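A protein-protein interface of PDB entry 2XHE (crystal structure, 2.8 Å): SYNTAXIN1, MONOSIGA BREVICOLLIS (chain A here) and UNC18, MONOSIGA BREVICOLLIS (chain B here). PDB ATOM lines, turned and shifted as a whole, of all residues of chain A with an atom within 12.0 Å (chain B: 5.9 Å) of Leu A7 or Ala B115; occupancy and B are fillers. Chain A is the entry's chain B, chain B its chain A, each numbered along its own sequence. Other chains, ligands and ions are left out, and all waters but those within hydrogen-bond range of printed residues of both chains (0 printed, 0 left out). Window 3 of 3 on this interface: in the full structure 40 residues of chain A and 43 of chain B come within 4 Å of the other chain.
Printed residues of chain B that touch a printed residue of chain A: Met B111, Ala B115, Val B120, Val B123 and Leu B126. Hydrophobic or aromatic side chains of chain B within 4 Å of the printed part of chain A: Met B111, Ala B115, Val B120 and Leu B126. Along chain A the printed residues that touch a printed residue of chain B span positions 3 to 14. Among the printed residues, 11 pairs touch across the chains.
NH2 of Arg A8 lies within hydrogen-bond range of O of Val B123 (3.4 Å).
Of chain A, only Leu A7, Met A10, Ala A11 and Asn A14 come within 4 Å of Ala B115. Of chain A, only Leu A7 comes within 4 Å of Met B111. No residue of chain A comes within 4 Å of Ala B112. No residue of chain A comes within 4 Å of Ser B116. No residue of chain A comes within 4 Å of Ala B117. Of the printed residues of chain A, Val B120 touches Leu A7 and Ala A11. Of chain A, only Arg A3 and Leu A4 come within 4 Å of Leu B126. Of the printed residues of chain B, Arg A8 touches Val B123. Of the printed residues of chain B, Arg A3 touches Leu B126. Printed residues of chain B within 4 Å of Met A10: Ala B115 (3.4 Å). Of the printed residues of chain B, Asn A14 touches Ala B115 (3.9 Å). Printed residues of chain B within 4 Å of Leu A4: Val B123 (3.8 Å) and Leu B126 (3.7 Å). Ala A12 touches none of the printed residues of chain B. The nearest residue of chain A that does not touch Ala B115 is Ala A12 (6.2 Å).
The backbone carbonyl oxygen (O) of Ala A11 lies close to the side-chain amide oxygen (OD1) of Asn A14, at 3.3 Å.
Among the printed residues, merely in contact across the chains: Arg A3 with Leu B126 (3.6 Å), Leu A4 with Val B123 (3.8 Å), Leu A4 with Leu B126 (3.7 Å), Leu A7 with Met B111 (3.6 Å), Leu A7 with Ala B115 (3.9 Å), Leu A7 with Val B120 (3.98 Å), Met A10 with Ala B115 (3.4 Å), Ala A11 with Ala B115 (3.7 Å), Ala A11 with Val B120 (3.4 Å) and Asn A14 with Ala B115 (3.9 Å).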
ATOM      1  N   ASP A   2      27.346  -1.504  25.157  1.00  0.00           N
ATOM      2  CA  ASP A   2      26.630  -2.259  24.133  1.00  0.00           C
ATOM      3  C   ASP A   2      25.372  -1.536  23.666  1.00  0.00           C
ATOM      4  O   ASP A   2      25.349  -0.955  22.580  1.00  0.00           O
ATOM      5  CB  ASP A   2      26.265  -3.659  24.639  1.00  0.00           C
ATOM      6  CG  ASP A   2      27.282  -4.715  24.231  1.00  0.00           C
ATOM      7  OD1 ASP A   2      28.297  -4.352  23.597  1.00  0.00           O
ATOM      8  OD2 ASP A   2      27.061  -5.906  24.540  1.00  0.00           O
ATOM      9  N   ARG A   3      24.329  -1.577  24.490  1.00  0.00           N
ATOM     10  CA  ARG A   3      23.038  -1.019  24.101  1.00  0.00           C
ATOM     11  C   ARG A   3      23.089   0.500  23.971  1.00  0.00           C
ATOM     12  O   ARG A   3      22.119   1.117  23.537  1.00  0.00           O
ATOM     13  CB  ARG A   3      21.930  -1.443  25.073  1.00  0.00           C
ATOM     14  CG  ARG A   3      21.952  -2.920  25.456  1.00  0.00           C
ATOM     15  CD  ARG A   3      22.776  -3.147  26.728  1.00  0.00           C
ATOM     16  NE  ARG A   3      22.997  -4.564  27.020  1.00  0.00           N
ATOM     17  CZ  ARG A   3      23.504  -5.026  28.162  1.00  0.00           C
ATOM     18  NH1 ARG A   3      23.833  -4.185  29.132  1.00  0.00           N
ATOM     19  NH2 ARG A   3      23.674  -6.329  28.339  1.00  0.00           N
ATOM     20  N   LEU A   4      24.219   1.098  24.350  1.00  0.00           N
ATOM     21  CA  LEU A   4      24.417   2.543  24.188  1.00  0.00           C
ATOM     22  C   LEU A   4      24.859   2.873  22.769  1.00  0.00           C
ATOM     23  O   LEU A   4      24.391   3.851  22.182  1.00  0.00           O
ATOM     24  CB  LEU A   4      25.430   3.086  25.207  1.00  0.00           C
ATOM     25  CG  LEU A   4      25.774   4.591  25.241  1.00  0.00           C
ATOM     26  CD1 LEU A   4      26.922   4.943  24.289  1.00  0.00           C
ATOM     27  CD2 LEU A   4      24.558   5.505  25.011  1.00  0.00           C
ATOM     28  N   SER A   5      25.763   2.060  22.223  1.00  0.00           N
ATOM     29  CA  SER A   5      26.173   2.202  20.830  1.00  0.00           C
ATOM     30  C   SER A   5      24.949   2.141  19.926  1.00  0.00           C
ATOM     31  O   SER A   5      24.738   3.023  19.093  1.00  0.00           O
ATOM     32  CB  SER A   5      27.166   1.104  20.430  1.00  0.00           C
ATOM     33  OG  SER A   5      28.474   1.376  20.908  1.00  0.00           O
ATOM     34  N   ARG A   6      24.142   1.099  20.114  1.00  0.00           N
ATOM     35  CA  ARG A   6      22.964   0.853  19.288  1.00  0.00           C
ATOM     36  C   ARG A   6      21.972   2.017  19.311  1.00  0.00           C
ATOM     37  O   ARG A   6      21.203   2.196  18.370  1.00  0.00           O
ATOM     38  CB  ARG A   6      22.266  -0.441  19.723  1.00  0.00           C
ATOM     39  CG  ARG A   6      23.154  -1.692  19.704  1.00  0.00           C
ATOM     40  CD  ARG A   6      22.482  -2.867  20.430  1.00  0.00           C
ATOM     41  NE  ARG A   6      23.348  -4.042  20.541  1.00  0.00           N
ATOM     42  CZ  ARG A   6      23.071  -5.116  21.279  1.00  0.00           C
ATOM     43  NH1 ARG A   6      21.947  -5.173  21.985  1.00  0.00           N
ATOM     44  NH2 ARG A   6      23.921  -6.134  21.316  1.00  0.00           N
ATOM     45  N   LEU A   7      21.991   2.802  20.386  1.00  0.00           N
ATOM     46  CA  LEU A   7      21.112   3.970  20.514  1.00  0.00           C
ATOM     47  C   LEU A   7      21.652   5.164  19.728  1.00  0.00           C
ATOM     48  O   LEU A   7      20.911   5.823  19.000  1.00  0.00           O
ATOM     49  CB  LEU A   7      20.910   4.349  21.994  1.00  0.00           C
ATOM     50  CG  LEU A   7      19.714   5.232  22.395  1.00  0.00           C
ATOM     51  CD1 LEU A   7      20.077   6.697  22.533  1.00  0.00           C
ATOM     52  CD2 LEU A   7      18.542   5.064  21.432  1.00  0.00           C
ATOM     53  N   ARG A   8      22.946   5.436  19.877  1.00  0.00           N
ATOM     54  CA  ARG A   8      23.573   6.567  19.200  1.00  0.00           C
ATOM     55  C   ARG A   8      23.670   6.341  17.690  1.00  0.00           C
ATOM     56  O   ARG A   8      23.743   7.294  16.910  1.00  0.00           O
ATOM     57  CB  ARG A   8      24.945   6.878  19.812  1.00  0.00           C
ATOM     58  CG  ARG A   8      24.895   7.861  20.982  1.00  0.00           C
ATOM     59  CD  ARG A   8      26.153   7.796  21.842  1.00  0.00           C
ATOM     60  NE  ARG A   8      26.123   8.777  22.925  1.00  0.00           N
ATOM     61  CZ  ARG A   8      27.035   8.852  23.891  1.00  0.00           C
ATOM     62  NH1 ARG A   8      28.045   7.994  23.912  1.00  0.00           N
ATOM     63  NH2 ARG A   8      26.938   9.782  24.836  1.00  0.00           N
ATOM     64  N   GLN A   9      23.669   5.077  17.282  1.00  0.00           N
ATOM     65  CA  GLN A   9      23.575   4.742  15.869  1.00  0.00           C
ATOM     66  C   GLN A   9      22.169   5.048  15.374  1.00  0.00           C
ATOM     67  O   GLN A   9      21.991   5.649  14.316  1.00  0.00           O
ATOM     68  CB  GLN A   9      23.890   3.264  15.640  1.00  0.00           C
ATOM     69  CG  GLN A   9      23.534   2.767  14.247  1.00  0.00           C
ATOM     70  CD  GLN A   9      23.515   1.250  14.155  1.00  0.00           C
ATOM     71  OE1 GLN A   9      23.903   0.556  15.096  1.00  0.00           O
ATOM     72  NE2 GLN A   9      23.058   0.729  13.017  1.00  0.00           N
ATOM     73  N   MET A  10      21.172   4.640  16.156  1.00  0.00           N
ATOM     74  CA  MET A  10      19.765   4.789  15.788  1.00  0.00           C
ATOM     75  C   MET A  10      19.225   6.206  16.021  1.00  0.00           C
ATOM     76  O   MET A  10      18.033   6.461  15.846  1.00  0.00           O
ATOM     77  CB  MET A  10      18.912   3.760  16.544  1.00  0.00           C
ATOM     78  CG  MET A  10      19.241   2.305  16.202  1.00  0.00           C
ATOM     79  SD  MET A  10      18.529   1.102  17.348  1.00  0.00           S
ATOM     80  CE  MET A  10      19.050  -0.440  16.583  1.00  0.00           C
ATOM     81  N   ALA A  11      20.105   7.123  16.410  1.00  0.00           N
ATOM     82  CA  ALA A  11      19.706   8.508  16.641  1.00  0.00           C
ATOM     83  C   ALA A  11      20.409   9.444  15.664  1.00  0.00           C
ATOM     84  O   ALA A  11      20.007  10.596  15.493  1.00  0.00           O
ATOM     85  CB  ALA A  11      20.000   8.915  18.074  1.00  0.00           C
ATOM     86  N   ALA A  12      21.462   8.935  15.029  1.00  0.00           N
ATOM     87  CA  ALA A  12      22.211   9.697  14.033  1.00  0.00           C
ATOM     88  C   ALA A  12      21.658   9.459  12.627  1.00  0.00           C
ATOM     89  O   ALA A  12      22.111  10.077  11.662  1.00  0.00           O
ATOM     90  CB  ALA A  12      23.694   9.347  14.095  1.00  0.00           C
ATOM     91  N   GLU A  13      20.682   8.560  12.524  1.00  0.00           N
ATOM     92  CA  GLU A  13      19.994   8.281  11.263  1.00  0.00           C
ATOM     93  C   GLU A  13      18.746   9.151  11.123  1.00  0.00           C
ATOM     94  O   GLU A  13      17.771   8.765  10.473  1.00  0.00           O
ATOM     95  CB  GLU A  13      19.597   6.804  11.178  1.00  0.00           C
ATOM     96  CG  GLU A  13      20.761   5.828  11.217  1.00  0.00           C
ATOM     97  CD  GLU A  13      20.300   4.380  11.250  1.00  0.00           C
ATOM     98  OE1 GLU A  13      19.071   4.149  11.262  1.00  0.00           O
ATOM     99  OE2 GLU A  13      21.165   3.478  11.268  1.00  0.00           O
ATOM    100  N   ASN A  14      18.785  10.323  11.749  1.00  0.00           N
ATOM    101  CA  ASN A  14      17.678  11.268  11.711  1.00  0.00           C
ATOM    102  C   ASN A  14      18.172  12.620  11.213  1.00  0.00           C
ATOM    103  O   ASN A  14      17.443  13.359  10.548  1.00  0.00           O
ATOM    104  CB  ASN A  14      17.061  11.417  13.105  1.00  0.00           C
ATOM    105  CG  ASN A  14      16.696  10.080  13.732  1.00  0.00           C
ATOM    106  OD1 ASN A  14      16.884   9.870  14.932  1.00  0.00           O
ATOM    107  ND2 ASN A  14      16.175   9.166  12.919  1.00  0.00           N
ATOM    108  N   GLN A  15      19.426  12.925  11.543  1.00  0.00           N
ATOM    109  CA  GLN A  15      20.070  14.171  11.141  1.00  0.00           C
ATOM    110  C   GLN A  15      20.881  13.987   9.858  1.00  0.00           C
ATOM    111  O   GLN A  15      22.063  13.644   9.901  1.00  0.00           O
ATOM    112  CB  GLN A  15      20.985  14.678  12.260  1.00  0.00           C
ATOM    113  CG  GLN A  15      20.310  14.790  13.620  1.00  0.00           C
ATOM    114  CD  GLN A  15      21.299  15.078  14.735  1.00  0.00           C
ATOM    115  OE1 GLN A  15      22.496  15.251  14.489  1.00  0.00           O
ATOM    116  NE2 GLN A  15      20.807  15.128  15.970  1.00  0.00           N
ATOM    117  N   LEU B 110      10.429   1.589  21.668  1.00  0.00           N
ATOM    118  CA  LEU B 110      10.710   2.570  22.716  1.00  0.00           C
ATOM    119  C   LEU B 110      12.089   3.187  22.525  1.00  0.00           C
ATOM    120  O   LEU B 110      12.263   4.399  22.669  1.00  0.00           O
ATOM    121  CB  LEU B 110      10.606   1.931  24.104  1.00  0.00           C
ATOM    122  CG  LEU B 110       9.197   1.615  24.624  1.00  0.00           C
ATOM    123  CD1 LEU B 110       8.360   2.888  24.677  1.00  0.00           C
ATOM    124  CD2 LEU B 110       8.494   0.535  23.790  1.00  0.00           C
ATOM    125  N   MET B 111      13.064   2.343  22.197  1.00  0.00           N
ATOM    126  CA  MET B 111      14.416   2.804  21.911  1.00  0.00           C
ATOM    127  C   MET B 111      14.356   3.932  20.882  1.00  0.00           C
ATOM    128  O   MET B 111      15.008   4.965  21.042  1.00  0.00           O
ATOM    129  CB  MET B 111      15.292   1.643  21.419  1.00  0.00           C
ATOM    130  CG  MET B 111      16.797   1.819  21.668  1.00  0.00           C
ATOM    131  SD  MET B 111      17.531   0.613  22.810  1.00  0.00           S
ATOM    132  CE  MET B 111      16.905  -0.925  22.116  1.00  0.00           C
ATOM    133  N   ALA B 112      13.550   3.742  19.842  1.00  0.00           N
ATOM    134  CA  ALA B 112      13.364   4.769  18.821  1.00  0.00           C
ATOM    135  C   ALA B 112      12.799   6.063  19.406  1.00  0.00           C
ATOM    136  O   ALA B 112      13.328   7.141  19.150  1.00  0.00           O
ATOM    137  CB  ALA B 112      12.474   4.261  17.700  1.00  0.00           C
ATOM    138  N   LYS B 113      11.731   5.955  20.191  1.00  0.00           N
ATOM    139  CA  LYS B 113      11.093   7.138  20.772  1.00  0.00           C
ATOM    140  C   LYS B 113      12.097   8.024  21.505  1.00  0.00           C
ATOM    141  O   LYS B 113      11.981   9.252  21.489  1.00  0.00           O
ATOM    142  CB  LYS B 113       9.952   6.745  21.719  1.00  0.00           C
ATOM    143  CG  LYS B 113       9.190   7.936  22.298  1.00  0.00           C
ATOM    144  CD  LYS B 113       7.880   7.502  22.942  1.00  0.00           C
ATOM    145  CE  LYS B 113       7.023   8.702  23.323  1.00  0.00           C
ATOM    146  NZ  LYS B 113       5.621   8.301  23.642  1.00  0.00           N
ATOM    147  N   LEU B 114      13.078   7.390  22.141  1.00  0.00           N
ATOM    148  CA  LEU B 114      14.124   8.096  22.874  1.00  0.00           C
ATOM    149  C   LEU B 114      15.110   8.747  21.910  1.00  0.00           C
ATOM    150  O   LEU B 114      15.563   9.869  22.132  1.00  0.00           O
ATOM    151  CB  LEU B 114      14.877   7.129  23.793  1.00  0.00           C
ATOM    152  CG  LEU B 114      15.405   7.633  25.143  1.00  0.00           C
ATOM    153  CD1 LEU B 114      16.606   6.811  25.592  1.00  0.00           C
ATOM    154  CD2 LEU B 114      15.773   9.097  25.086  1.00  0.00           C
ATOM    155  N   ALA B 115      15.442   8.030  20.840  1.00  0.00           N
ATOM    156  CA  ALA B 115      16.418   8.506  19.861  1.00  0.00           C
ATOM    157  C   ALA B 115      15.965   9.775  19.133  1.00  0.00           C
ATOM    158  O   ALA B 115      16.793  10.604  18.750  1.00  0.00           O
ATOM    159  CB  ALA B 115      16.750   7.402  18.859  1.00  0.00           C
ATOM    160  N   SER B 116      14.655   9.924  18.946  1.00  0.00           N
ATOM    161  CA  SER B 116      14.115  11.068  18.212  1.00  0.00           C
ATOM    162  C   SER B 116      13.990  12.318  19.082  1.00  0.00           C
ATOM    163  O   SER B 116      14.141  13.437  18.596  1.00  0.00           O
ATOM    164  CB  SER B 116      12.760  10.725  17.587  1.00  0.00           C
ATOM    165  OG  SER B 116      11.782  10.492  18.584  1.00  0.00           O
ATOM    166  N   ALA B 117      13.716  12.122  20.366  1.00  0.00           N
ATOM    167  CA  ALA B 117      13.568  13.237  21.299  1.00  0.00           C
ATOM    168  C   ALA B 117      14.916  13.855  21.663  1.00  0.00           C
ATOM    169  O   ALA B 117      15.958  13.208  21.544  1.00  0.00           O
ATOM    170  CB  ALA B 117      12.828  12.789  22.559  1.00  0.00           C
ATOM    171  N   VAL B 120      18.269  12.403  23.695  1.00  0.00           N
ATOM    172  CA  VAL B 120      19.314  11.531  23.173  1.00  0.00           C
ATOM    173  C   VAL B 120      20.725  12.072  23.433  1.00  0.00           C
ATOM    174  O   VAL B 120      21.632  11.314  23.783  1.00  0.00           O
ATOM    175  CB  VAL B 120      19.100  11.217  21.677  1.00  0.00           C
ATOM    176  CG1 VAL B 120      18.885  12.492  20.882  1.00  0.00           C
ATOM    177  CG2 VAL B 120      20.269  10.412  21.119  1.00  0.00           C
ATOM    178  N   VAL B 123      22.027  11.316  27.103  1.00  0.00           N
ATOM    179  CA  VAL B 123      22.152   9.969  27.652  1.00  0.00           C
ATOM    180  C   VAL B 123      23.556   9.394  27.441  1.00  0.00           C
ATOM    181  O   VAL B 123      23.941   9.030  26.331  1.00  0.00           O
ATOM    182  CB  VAL B 123      20.986   9.011  27.190  1.00  0.00           C
ATOM    183  CG1 VAL B 123      20.523   9.352  25.792  1.00  0.00           C
ATOM    184  CG2 VAL B 123      21.375   7.535  27.303  1.00  0.00           C
ATOM    185  N   LEU B 126      23.920   3.316  28.862  1.00  0.00           N
ATOM    186  CA  LEU B 126      22.567   2.751  28.848  1.00  0.00           C
ATOM    187  C   LEU B 126      22.668   1.229  28.849  1.00  0.00           C
ATOM    188  O   LEU B 126      22.996   0.625  27.831  1.00  0.00           O
ATOM    189  CB  LEU B 126      21.783   3.234  27.621  1.00  0.00           C
ATOM    190  CG  LEU B 126      20.324   2.800  27.397  1.00  0.00           C
ATOM    191  CD1 LEU B 126      19.609   3.759  26.460  1.00  0.00           C
ATOM    192  CD2 LEU B 126      20.209   1.377  26.860  1.00  0.00           C
